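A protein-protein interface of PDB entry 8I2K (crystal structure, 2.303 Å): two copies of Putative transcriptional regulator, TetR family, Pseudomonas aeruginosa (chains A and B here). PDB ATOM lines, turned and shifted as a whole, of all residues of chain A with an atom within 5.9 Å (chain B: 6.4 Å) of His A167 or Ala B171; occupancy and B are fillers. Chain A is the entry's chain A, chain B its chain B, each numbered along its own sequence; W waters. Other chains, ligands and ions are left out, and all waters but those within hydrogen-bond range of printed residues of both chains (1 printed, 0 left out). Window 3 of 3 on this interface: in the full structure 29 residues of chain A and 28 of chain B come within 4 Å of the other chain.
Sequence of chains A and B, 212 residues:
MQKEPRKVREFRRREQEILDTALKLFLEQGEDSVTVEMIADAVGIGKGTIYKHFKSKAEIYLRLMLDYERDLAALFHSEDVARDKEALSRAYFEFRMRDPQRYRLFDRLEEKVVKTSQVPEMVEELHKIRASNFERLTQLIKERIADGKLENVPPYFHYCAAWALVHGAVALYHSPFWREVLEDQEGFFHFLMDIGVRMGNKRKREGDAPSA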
ATOM      1  N   TYR A 103      -1.588 -13.967   0.877  1.00  0.00           N
ATOM      2  CA  TYR A 103      -2.407 -13.315  -0.149  1.00  0.00           C
ATOM      3  C   TYR A 103      -3.835 -13.821  -0.075  1.00  0.00           C
ATOM      4  O   TYR A 103      -4.798 -13.049  -0.015  1.00  0.00           O
ATOM      5  CB  TYR A 103      -1.815 -13.580  -1.545  1.00  0.00           C
ATOM      6  CG  TYR A 103      -2.591 -12.941  -2.682  1.00  0.00           C
ATOM      7  CD1 TYR A 103      -3.824 -13.441  -3.059  1.00  0.00           C
ATOM      8  CD2 TYR A 103      -2.108 -11.811  -3.344  1.00  0.00           C
ATOM      9  CE1 TYR A 103      -4.546 -12.854  -4.066  1.00  0.00           C
ATOM     10  CE2 TYR A 103      -2.831 -11.212  -4.344  1.00  0.00           C
ATOM     11  CZ  TYR A 103      -4.037 -11.741  -4.711  1.00  0.00           C
ATOM     12  OH  TYR A 103      -4.732 -11.168  -5.741  1.00  0.00           O
ATOM     13  N   ARG A 104      -3.970 -15.130  -0.007  1.00  0.00           N
ATOM     14  CA  ARG A 104      -5.270 -15.770  -0.007  1.00  0.00           C
ATOM     15  C   ARG A 104      -6.018 -15.510   1.279  1.00  0.00           C
ATOM     16  O   ARG A 104      -7.229 -15.330   1.253  1.00  0.00           O
ATOM     17  CB  ARG A 104      -5.079 -17.268  -0.216  1.00  0.00           C
ATOM     18  CG  ARG A 104      -6.336 -18.066  -0.184  1.00  0.00           C
ATOM     19  CD  ARG A 104      -6.188 -19.191  -1.218  1.00  0.00           C
ATOM     20  NE  ARG A 104      -6.107 -18.637  -2.569  1.00  0.00           N
ATOM     21  CZ  ARG A 104      -6.519 -19.258  -3.674  1.00  0.00           C
ATOM     22  NH1 ARG A 104      -7.050 -20.478  -3.615  1.00  0.00           N
ATOM     23  NH2 ARG A 104      -6.387 -18.651  -4.849  1.00  0.00           N
ATOM     24  N   ASP A 107      -7.441 -12.060   1.085  1.00  0.00           N
ATOM     25  CA  ASP A 107      -8.669 -12.040   0.298  1.00  0.00           C
ATOM     26  C   ASP A 107      -9.874 -12.406   1.144  1.00  0.00           C
ATOM     27  O   ASP A 107     -10.948 -11.815   1.001  1.00  0.00           O
ATOM     28  CB  ASP A 107      -8.587 -13.009  -0.877  1.00  0.00           C
ATOM     29  CG  ASP A 107      -8.090 -12.369  -2.135  1.00  0.00           C
ATOM     30  OD1 ASP A 107      -7.830 -11.148  -2.156  1.00  0.00           O
ATOM     31  OD2 ASP A 107      -7.963 -13.112  -3.123  1.00  0.00           O
ATOM     32  N   ALA A 162      -0.670  -6.393 -13.967  1.00  0.00           N
ATOM     33  CA  ALA A 162       0.107  -6.826 -12.812  1.00  0.00           C
ATOM     34  C   ALA A 162      -0.770  -7.545 -11.805  1.00  0.00           C
ATOM     35  O   ALA A 162      -0.394  -8.599 -11.275  1.00  0.00           O
ATOM     36  CB  ALA A 162       0.787  -5.642 -12.130  1.00  0.00           C
ATOM     37  N   TRP A 163      -1.920  -6.947 -11.490  1.00  0.00           N
ATOM     38  CA  TRP A 163      -2.873  -7.558 -10.575  1.00  0.00           C
ATOM     39  C   TRP A 163      -3.274  -8.949 -11.061  1.00  0.00           C
ATOM     40  O   TRP A 163      -3.286  -9.914 -10.288  1.00  0.00           O
ATOM     41  CB  TRP A 163      -4.101  -6.659 -10.459  1.00  0.00           C
ATOM     42  CG  TRP A 163      -5.014  -7.055  -9.395  1.00  0.00           C
ATOM     43  CD1 TRP A 163      -5.082  -6.507  -8.156  1.00  0.00           C
ATOM     44  CD2 TRP A 163      -6.020  -8.081  -9.442  1.00  0.00           C
ATOM     45  NE1 TRP A 163      -6.031  -7.147  -7.406  1.00  0.00           N
ATOM     46  CE2 TRP A 163      -6.644  -8.101  -8.178  1.00  0.00           C
ATOM     47  CE3 TRP A 163      -6.460  -8.965 -10.423  1.00  0.00           C
ATOM     48  CZ2 TRP A 163      -7.688  -8.979  -7.868  1.00  0.00           C
ATOM     49  CZ3 TRP A 163      -7.471  -9.857 -10.114  1.00  0.00           C
ATOM     50  CH2 TRP A 163      -8.077  -9.862  -8.844  1.00  0.00           C
ATOM     51  N   ALA A 164      -3.613  -9.068 -12.343  1.00  0.00           N
ATOM     52  CA  ALA A 164      -4.032 -10.359 -12.865  1.00  0.00           C
ATOM     53  C   ALA A 164      -2.924 -11.392 -12.716  1.00  0.00           C
ATOM     54  O   ALA A 164      -3.176 -12.536 -12.326  1.00  0.00           O
ATOM     55  CB  ALA A 164      -4.458 -10.228 -14.327  1.00  0.00           C
ATOM     56  N   LEU A 165      -1.694 -11.016 -13.052  1.00  0.00           N
ATOM     57  CA  LEU A 165      -0.596 -11.971 -13.018  1.00  0.00           C
ATOM     58  C   LEU A 165      -0.366 -12.479 -11.607  1.00  0.00           C
ATOM     59  O   LEU A 165      -0.235 -13.686 -11.382  1.00  0.00           O
ATOM     60  CB  LEU A 165       0.662 -11.325 -13.582  1.00  0.00           C
ATOM     61  CG  LEU A 165       1.832 -12.310 -13.663  1.00  0.00           C
ATOM     62  CD1 LEU A 165       1.634 -13.379 -14.721  1.00  0.00           C
ATOM     63  CD2 LEU A 165       3.132 -11.593 -13.930  1.00  0.00           C
ATOM     64  N   VAL A 166      -0.329 -11.562 -10.639  1.00  0.00           N
ATOM     65  CA  VAL A 166      -0.153 -11.956  -9.252  1.00  0.00           C
ATOM     66  C   VAL A 166      -1.304 -12.858  -8.811  1.00  0.00           C
ATOM     67  O   VAL A 166      -1.094 -13.917  -8.195  1.00  0.00           O
ATOM     68  CB  VAL A 166      -0.028 -10.710  -8.365  1.00  0.00           C
ATOM     69  CG1 VAL A 166      -0.122 -11.128  -6.906  1.00  0.00           C
ATOM     70  CG2 VAL A 166       1.254  -9.957  -8.676  1.00  0.00           C
ATOM     71  N   HIS A 167      -2.540 -12.480  -9.165  1.00  0.00           N
ATOM     72  CA  HIS A 167      -3.686 -13.238  -8.702  1.00  0.00           C
ATOM     73  C   HIS A 167      -3.621 -14.686  -9.179  1.00  0.00           C
ATOM     74  O   HIS A 167      -3.805 -15.619  -8.391  1.00  0.00           O
ATOM     75  CB  HIS A 167      -4.987 -12.608  -9.163  1.00  0.00           C
ATOM     76  CG  HIS A 167      -6.169 -13.155  -8.434  1.00  0.00           C
ATOM     77  ND1 HIS A 167      -6.511 -12.723  -7.182  1.00  0.00           N
ATOM     78  CD2 HIS A 167      -6.994 -14.189  -8.711  1.00  0.00           C
ATOM     79  CE1 HIS A 167      -7.555 -13.409  -6.754  1.00  0.00           C
ATOM     80  NE2 HIS A 167      -7.876 -14.293  -7.674  1.00  0.00           N
ATOM     81  N   GLY A 168      -3.341 -14.890 -10.466  1.00  0.00           N
ATOM     82  CA  GLY A 168      -3.279 -16.238 -11.008  1.00  0.00           C
ATOM     83  C   GLY A 168      -2.056 -17.004 -10.546  1.00  0.00           C
ATOM     84  O   GLY A 168      -2.108 -18.221 -10.346  1.00  0.00           O
ATOM     85  N   ALA A 169      -0.938 -16.307 -10.354  1.00  0.00           N
ATOM     86  CA  ALA A 169       0.229 -16.959  -9.765  1.00  0.00           C
ATOM     87  C   ALA A 169      -0.104 -17.538  -8.395  1.00  0.00           C
ATOM     88  O   ALA A 169       0.272 -18.673  -8.081  1.00  0.00           O
ATOM     89  CB  ALA A 169       1.370 -15.973  -9.666  1.00  0.00           C
ATOM     90  N   VAL A 170      -0.845 -16.789  -7.581  1.00  0.00           N
ATOM     91  CA  VAL A 170      -1.236 -17.297  -6.274  1.00  0.00           C
ATOM     92  C   VAL A 170      -2.181 -18.485  -6.421  1.00  0.00           C
ATOM     93  O   VAL A 170      -2.045 -19.487  -5.724  1.00  0.00           O
ATOM     94  CB  VAL A 170      -1.849 -16.156  -5.434  1.00  0.00           C
ATOM     95  CG1 VAL A 170      -2.551 -16.691  -4.233  1.00  0.00           C
ATOM     96  CG2 VAL A 170      -0.770 -15.192  -5.034  1.00  0.00           C
ATOM     97  N   ALA A 171      -3.144 -18.402  -7.325  1.00  0.00           N
ATOM     98  CA  ALA A 171      -4.044 -19.532  -7.536  1.00  0.00           C
ATOM     99  C   ALA A 171      -3.300 -20.759  -8.040  1.00  0.00           C
ATOM    100  O   ALA A 171      -3.705 -21.892  -7.768  1.00  0.00           O
ATOM    101  CB  ALA A 171      -5.144 -19.169  -8.533  1.00  0.00           C
ATOM    102  N   LEU A 172      -2.253 -20.542  -8.822  1.00  0.00           N
ATOM    103  CA  LEU A 172      -1.446 -21.638  -9.340  1.00  0.00           C
ATOM    104  C   LEU A 172      -0.835 -22.442  -8.211  1.00  0.00           C
ATOM    105  O   LEU A 172      -0.795 -23.679  -8.260  1.00  0.00           O
ATOM    106  CB  LEU A 172      -0.355 -21.046 -10.219  1.00  0.00           C
ATOM    107  CG  LEU A 172       0.447 -21.934 -11.123  1.00  0.00           C
ATOM    108  CD1 LEU A 172      -0.492 -22.499 -12.109  1.00  0.00           C
ATOM    109  CD2 LEU A 172       1.476 -21.051 -11.744  1.00  0.00           C
ATOM    110  N   PRO B 100     -15.367 -14.347 -19.394  1.00  0.00           N
ATOM    111  CA  PRO B 100     -14.909 -14.797 -18.075  1.00  0.00           C
ATOM    112  C   PRO B 100     -16.008 -15.380 -17.236  1.00  0.00           C
ATOM    113  O   PRO B 100     -15.715 -16.226 -16.392  1.00  0.00           O
ATOM    114  CB  PRO B 100     -14.335 -13.522 -17.440  1.00  0.00           C
ATOM    115  CG  PRO B 100     -14.914 -12.399 -18.240  1.00  0.00           C
ATOM    116  CD  PRO B 100     -15.069 -12.927 -19.640  1.00  0.00           C
ATOM    117  N   ARG B 104     -15.957 -19.042 -15.185  1.00  0.00           N
ATOM    118  CA  ARG B 104     -16.210 -19.253 -13.770  1.00  0.00           C
ATOM    119  C   ARG B 104     -17.287 -20.286 -13.532  1.00  0.00           C
ATOM    120  O   ARG B 104     -17.217 -21.051 -12.570  1.00  0.00           O
ATOM    121  CB  ARG B 104     -16.641 -17.949 -13.107  1.00  0.00           C
ATOM    122  CG  ARG B 104     -15.521 -17.139 -12.668  1.00  0.00           C
ATOM    123  CD  ARG B 104     -15.574 -16.857 -11.181  1.00  0.00           C
ATOM    124  NE  ARG B 104     -14.264 -16.344 -10.824  1.00  0.00           N
ATOM    125  CZ  ARG B 104     -14.040 -15.262 -10.111  1.00  0.00           C
ATOM    126  NH1 ARG B 104     -15.040 -14.543  -9.608  1.00  0.00           N
ATOM    127  NH2 ARG B 104     -12.792 -14.905  -9.889  1.00  0.00           N
ATOM    128  N   ALA B 164      -1.986 -18.980 -15.303  1.00  0.00           N
ATOM    129  CA  ALA B 164      -2.062 -17.941 -14.283  1.00  0.00           C
ATOM    130  C   ALA B 164      -2.575 -16.619 -14.866  1.00  0.00           C
ATOM    131  O   ALA B 164      -3.485 -15.988 -14.297  1.00  0.00           O
ATOM    132  CB  ALA B 164      -0.691 -17.771 -13.643  1.00  0.00           C
ATOM    133  N   VAL B 166      -4.479 -16.207 -17.534  1.00  0.00           N
ATOM    134  CA  VAL B 166      -5.899 -16.360 -17.823  1.00  0.00           C
ATOM    135  C   VAL B 166      -6.718 -16.356 -16.539  1.00  0.00           C
ATOM    136  O   VAL B 166      -7.730 -15.665 -16.424  1.00  0.00           O
ATOM    137  CB  VAL B 166      -6.147 -17.654 -18.614  1.00  0.00           C
ATOM    138  CG1 VAL B 166      -7.644 -17.907 -18.651  1.00  0.00           C
ATOM    139  CG2 VAL B 166      -5.568 -17.533 -19.997  1.00  0.00           C
ATOM    140  N   HIS B 167      -6.304 -17.145 -15.559  1.00  0.00           N
ATOM    141  CA  HIS B 167      -7.052 -17.208 -14.316  1.00  0.00           C
ATOM    142  C   HIS B 167      -7.154 -15.835 -13.648  1.00  0.00           C
ATOM    143  O   HIS B 167      -8.216 -15.439 -13.154  1.00  0.00           O
ATOM    144  CB  HIS B 167      -6.392 -18.193 -13.366  1.00  0.00           C
ATOM    145  CG  HIS B 167      -7.266 -18.569 -12.218  1.00  0.00           C
ATOM    146  ND1 HIS B 167      -8.320 -19.449 -12.353  1.00  0.00           N
ATOM    147  CD2 HIS B 167      -7.257 -18.181 -10.917  1.00  0.00           C
ATOM    148  CE1 HIS B 167      -8.932 -19.577 -11.185  1.00  0.00           C
ATOM    149  NE2 HIS B 167      -8.284 -18.847 -10.292  1.00  0.00           N
ATOM    150  N   GLY B 168      -6.038 -15.118 -13.573  1.00  0.00           N
ATOM    151  CA  GLY B 168      -6.056 -13.812 -12.940  1.00  0.00           C
ATOM    152  C   GLY B 168      -6.830 -12.809 -13.753  1.00  0.00           C
ATOM    153  O   GLY B 168      -7.478 -11.917 -13.194  1.00  0.00           O
ATOM    154  N   ALA B 169      -6.796 -12.956 -15.085  1.00  0.00           N
ATOM    155  CA  ALA B 169      -7.610 -12.110 -15.947  1.00  0.00           C
ATOM    156  C   ALA B 169      -9.104 -12.280 -15.666  1.00  0.00           C
ATOM    157  O   ALA B 169      -9.848 -11.289 -15.613  1.00  0.00           O
ATOM    158  CB  ALA B 169      -7.293 -12.435 -17.396  1.00  0.00           C
ATOM    159  N   VAL B 170      -9.564 -13.534 -15.527  1.00  0.00           N
ATOM    160  CA  VAL B 170     -10.973 -13.790 -15.261  1.00  0.00           C
ATOM    161  C   VAL B 170     -11.377 -13.183 -13.928  1.00  0.00           C
ATOM    162  O   VAL B 170     -12.433 -12.565 -13.810  1.00  0.00           O
ATOM    163  CB  VAL B 170     -11.259 -15.303 -15.295  1.00  0.00           C
ATOM    164  CG1 VAL B 170     -12.666 -15.568 -14.799  1.00  0.00           C
ATOM    165  CG2 VAL B 170     -11.056 -15.836 -16.676  1.00  0.00           C
ATOM    166  N   ALA B 171     -10.545 -13.340 -12.912  1.00  0.00           N
ATOM    167  CA  ALA B 171     -10.827 -12.698 -11.622  1.00  0.00           C
ATOM    168  C   ALA B 171     -10.861 -11.180 -11.750  1.00  0.00           C
ATOM    169  O   ALA B 171     -11.703 -10.514 -11.129  1.00  0.00           O
ATOM    170  CB  ALA B 171      -9.778 -13.094 -10.595  1.00  0.00           C
ATOM    171  N   LEU B 172      -9.920 -10.608 -12.510  1.00  0.00           N
ATOM    172  CA  LEU B 172      -9.919  -9.160 -12.733  1.00  0.00           C
ATOM    173  C   LEU B 172     -11.261  -8.682 -13.291  1.00  0.00           C
ATOM    174  O   LEU B 172     -11.792  -7.660 -12.836  1.00  0.00           O
ATOM    175  CB  LEU B 172      -8.758  -8.796 -13.665  1.00  0.00           C
ATOM    176  CG  LEU B 172      -8.723  -7.444 -14.359  1.00  0.00           C
ATOM    177  CD1 LEU B 172      -8.439  -6.311 -13.330  1.00  0.00           C
ATOM    178  CD2 LEU B 172      -7.657  -7.391 -15.438  1.00  0.00           C
ATOM    179  N   TYR B 173     -11.844  -9.440 -14.238  1.00  0.00           N
ATOM    180  CA  TYR B 173     -13.115  -9.101 -14.878  1.00  0.00           C
ATOM    181  C   TYR B 173     -14.305  -9.264 -13.942  1.00  0.00           C
ATOM    182  O   TYR B 173     -15.411  -8.857 -14.292  1.00  0.00           O
ATOM    183  CB  TYR B 173     -13.333  -9.975 -16.136  1.00  0.00           C
ATOM    184  CG  TYR B 173     -12.554  -9.472 -17.339  1.00  0.00           C
ATOM    185  CD1 TYR B 173     -11.387 -10.109 -17.775  1.00  0.00           C
ATOM    186  CD2 TYR B 173     -12.973  -8.352 -18.032  1.00  0.00           C
ATOM    187  CE1 TYR B 173     -10.676  -9.629 -18.854  1.00  0.00           C
ATOM    188  CE2 TYR B 173     -12.275  -7.868 -19.117  1.00  0.00           C
ATOM    189  CZ  TYR B 173     -11.128  -8.504 -19.516  1.00  0.00           C
ATOM    190  OH  TYR B 173     -10.459  -8.011 -20.606  1.00  0.00           O
ATOM    191  N   HIS B 174     -14.107  -9.877 -12.778  1.00  0.00           N
ATOM    192  CA  HIS B 174     -15.111  -9.935 -11.730  1.00  0.00           C
ATOM    193  C   HIS B 174     -14.859  -8.915 -10.612  1.00  0.00           C
ATOM    194  O   HIS B 174     -15.541  -8.955  -9.599  1.00  0.00           O
ATOM    195  CB  HIS B 174     -15.158 -11.362 -11.163  1.00  0.00           C
ATOM    196  CG  HIS B 174     -15.784 -12.360 -12.092  1.00  0.00           C
ATOM    197  ND1 HIS B 174     -15.075 -12.992 -13.091  1.00  0.00           N
ATOM    198  CD2 HIS B 174     -17.058 -12.823 -12.181  1.00  0.00           C
ATOM    199  CE1 HIS B 174     -15.885 -13.794 -13.769  1.00  0.00           C
ATOM    200  NE2 HIS B 174     -17.089 -13.720 -13.231  1.00  0.00           N
ATOM    201  N   SER B 175     -13.996  -8.017 -10.785  1.00  0.00           N
ATOM    202  CA  SER B 175     -13.567  -7.240  -9.636  1.00  0.00           C
ATOM    203  C   SER B 175     -14.198  -5.850  -9.611  1.00  0.00           C
ATOM    204  O   SER B 175     -14.474  -5.246 -10.664  1.00  0.00           O
ATOM    205  CB  SER B 175     -12.041  -7.083  -9.630  1.00  0.00           C
ATOM    206  OG  SER B 175     -11.689  -6.115 -10.597  1.00  0.00           O
HETATM  207  O   HOH W   1      -9.762 -16.277  -8.704  1.00  0.00           O
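The side-chain hydroxyl (OH) of Tyr A103 sits at hydrogen-bond distance from a ring nitrogen (ND1) of His A167 (2.8 Å). O of Leu B172 is in hydrogen-bond range of OG of Ser B175, 2.7 Å away.
Ala A164 touches its own counterpart, Ala B164. Ala A164 touches Ala B169, and with the chains exchanged Ala A169 touches Ala B164. His A167 touches Ala B171, and with the chains exchanged Ala A171 touches His B167. Gly B168 touches its own counterpart, Gly A168. 9 positions are printed for both chains.
Of the 13 printed residues of chain B, 6 touch a printed residue of chain A. Printed residues of chain B that touch a printed residue of chain A: Ala B164, His B167, Gly B168, Ala B169, Ala B171 and Leu B172. Hydrophobic or aromatic side chains of chain B that line the printed part of chain A: Ala B164, His B167, Ala B171 and Leu B172. Among the printed residues, 11 pairs touch across the chains. Among the printed residues, no Asp or Glu carboxylate lies within 4 Å of a Lys or Arg side-chain nitrogen of the other chain.
His A167 touches one residue of chain B. Printed residues of chain B within 4 Å of Ala A164: Ala B164 (3.99 Å), Gly B168 (3.2 Å) and Ala B169 (3.7 Å). Of the printed residues of chain A, His B167 touches Ala A171. Printed residues of chain B within 4 Å of Ala A169: Ala B164. Printed residues of chain B within 4 Å of Ala A171: His B167. Of the printed residues of chain A, Ala B164 touches Ala A164 (3.99 Å), Gly A168 (3.3 Å) and Ala A169 (3.6 Å). Tyr A103 touches none of the printed residues of chain B. The nearest printed residue of chain A that does not touch Leu B172 is Ala A164 (4.4 Å).
Among the printed residues, merely in contact across the chains: Trp A163 with Gly B168 (3.7 Å), Trp A163 with Ala B171 (3.99 Å), Trp A163 with Leu B172 (3.5 Å), Ala A164 with Ala B164 (3.99 Å), Ala A164 with Gly B168 (3.2 Å), Ala A164 with Ala B169 (3.7 Å), His A167 with Ala B171 (3.5 Å), Gly A168 with Ala B164 (3.3 Å), Gly A168 with Gly B168 (3.8 Å), Ala A169 with Ala B164 (3.6 Å) and Ala A171 with His B167 (3.3 Å).
Water W1 bridges NE2 of His A167 and NE2 of His B167.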
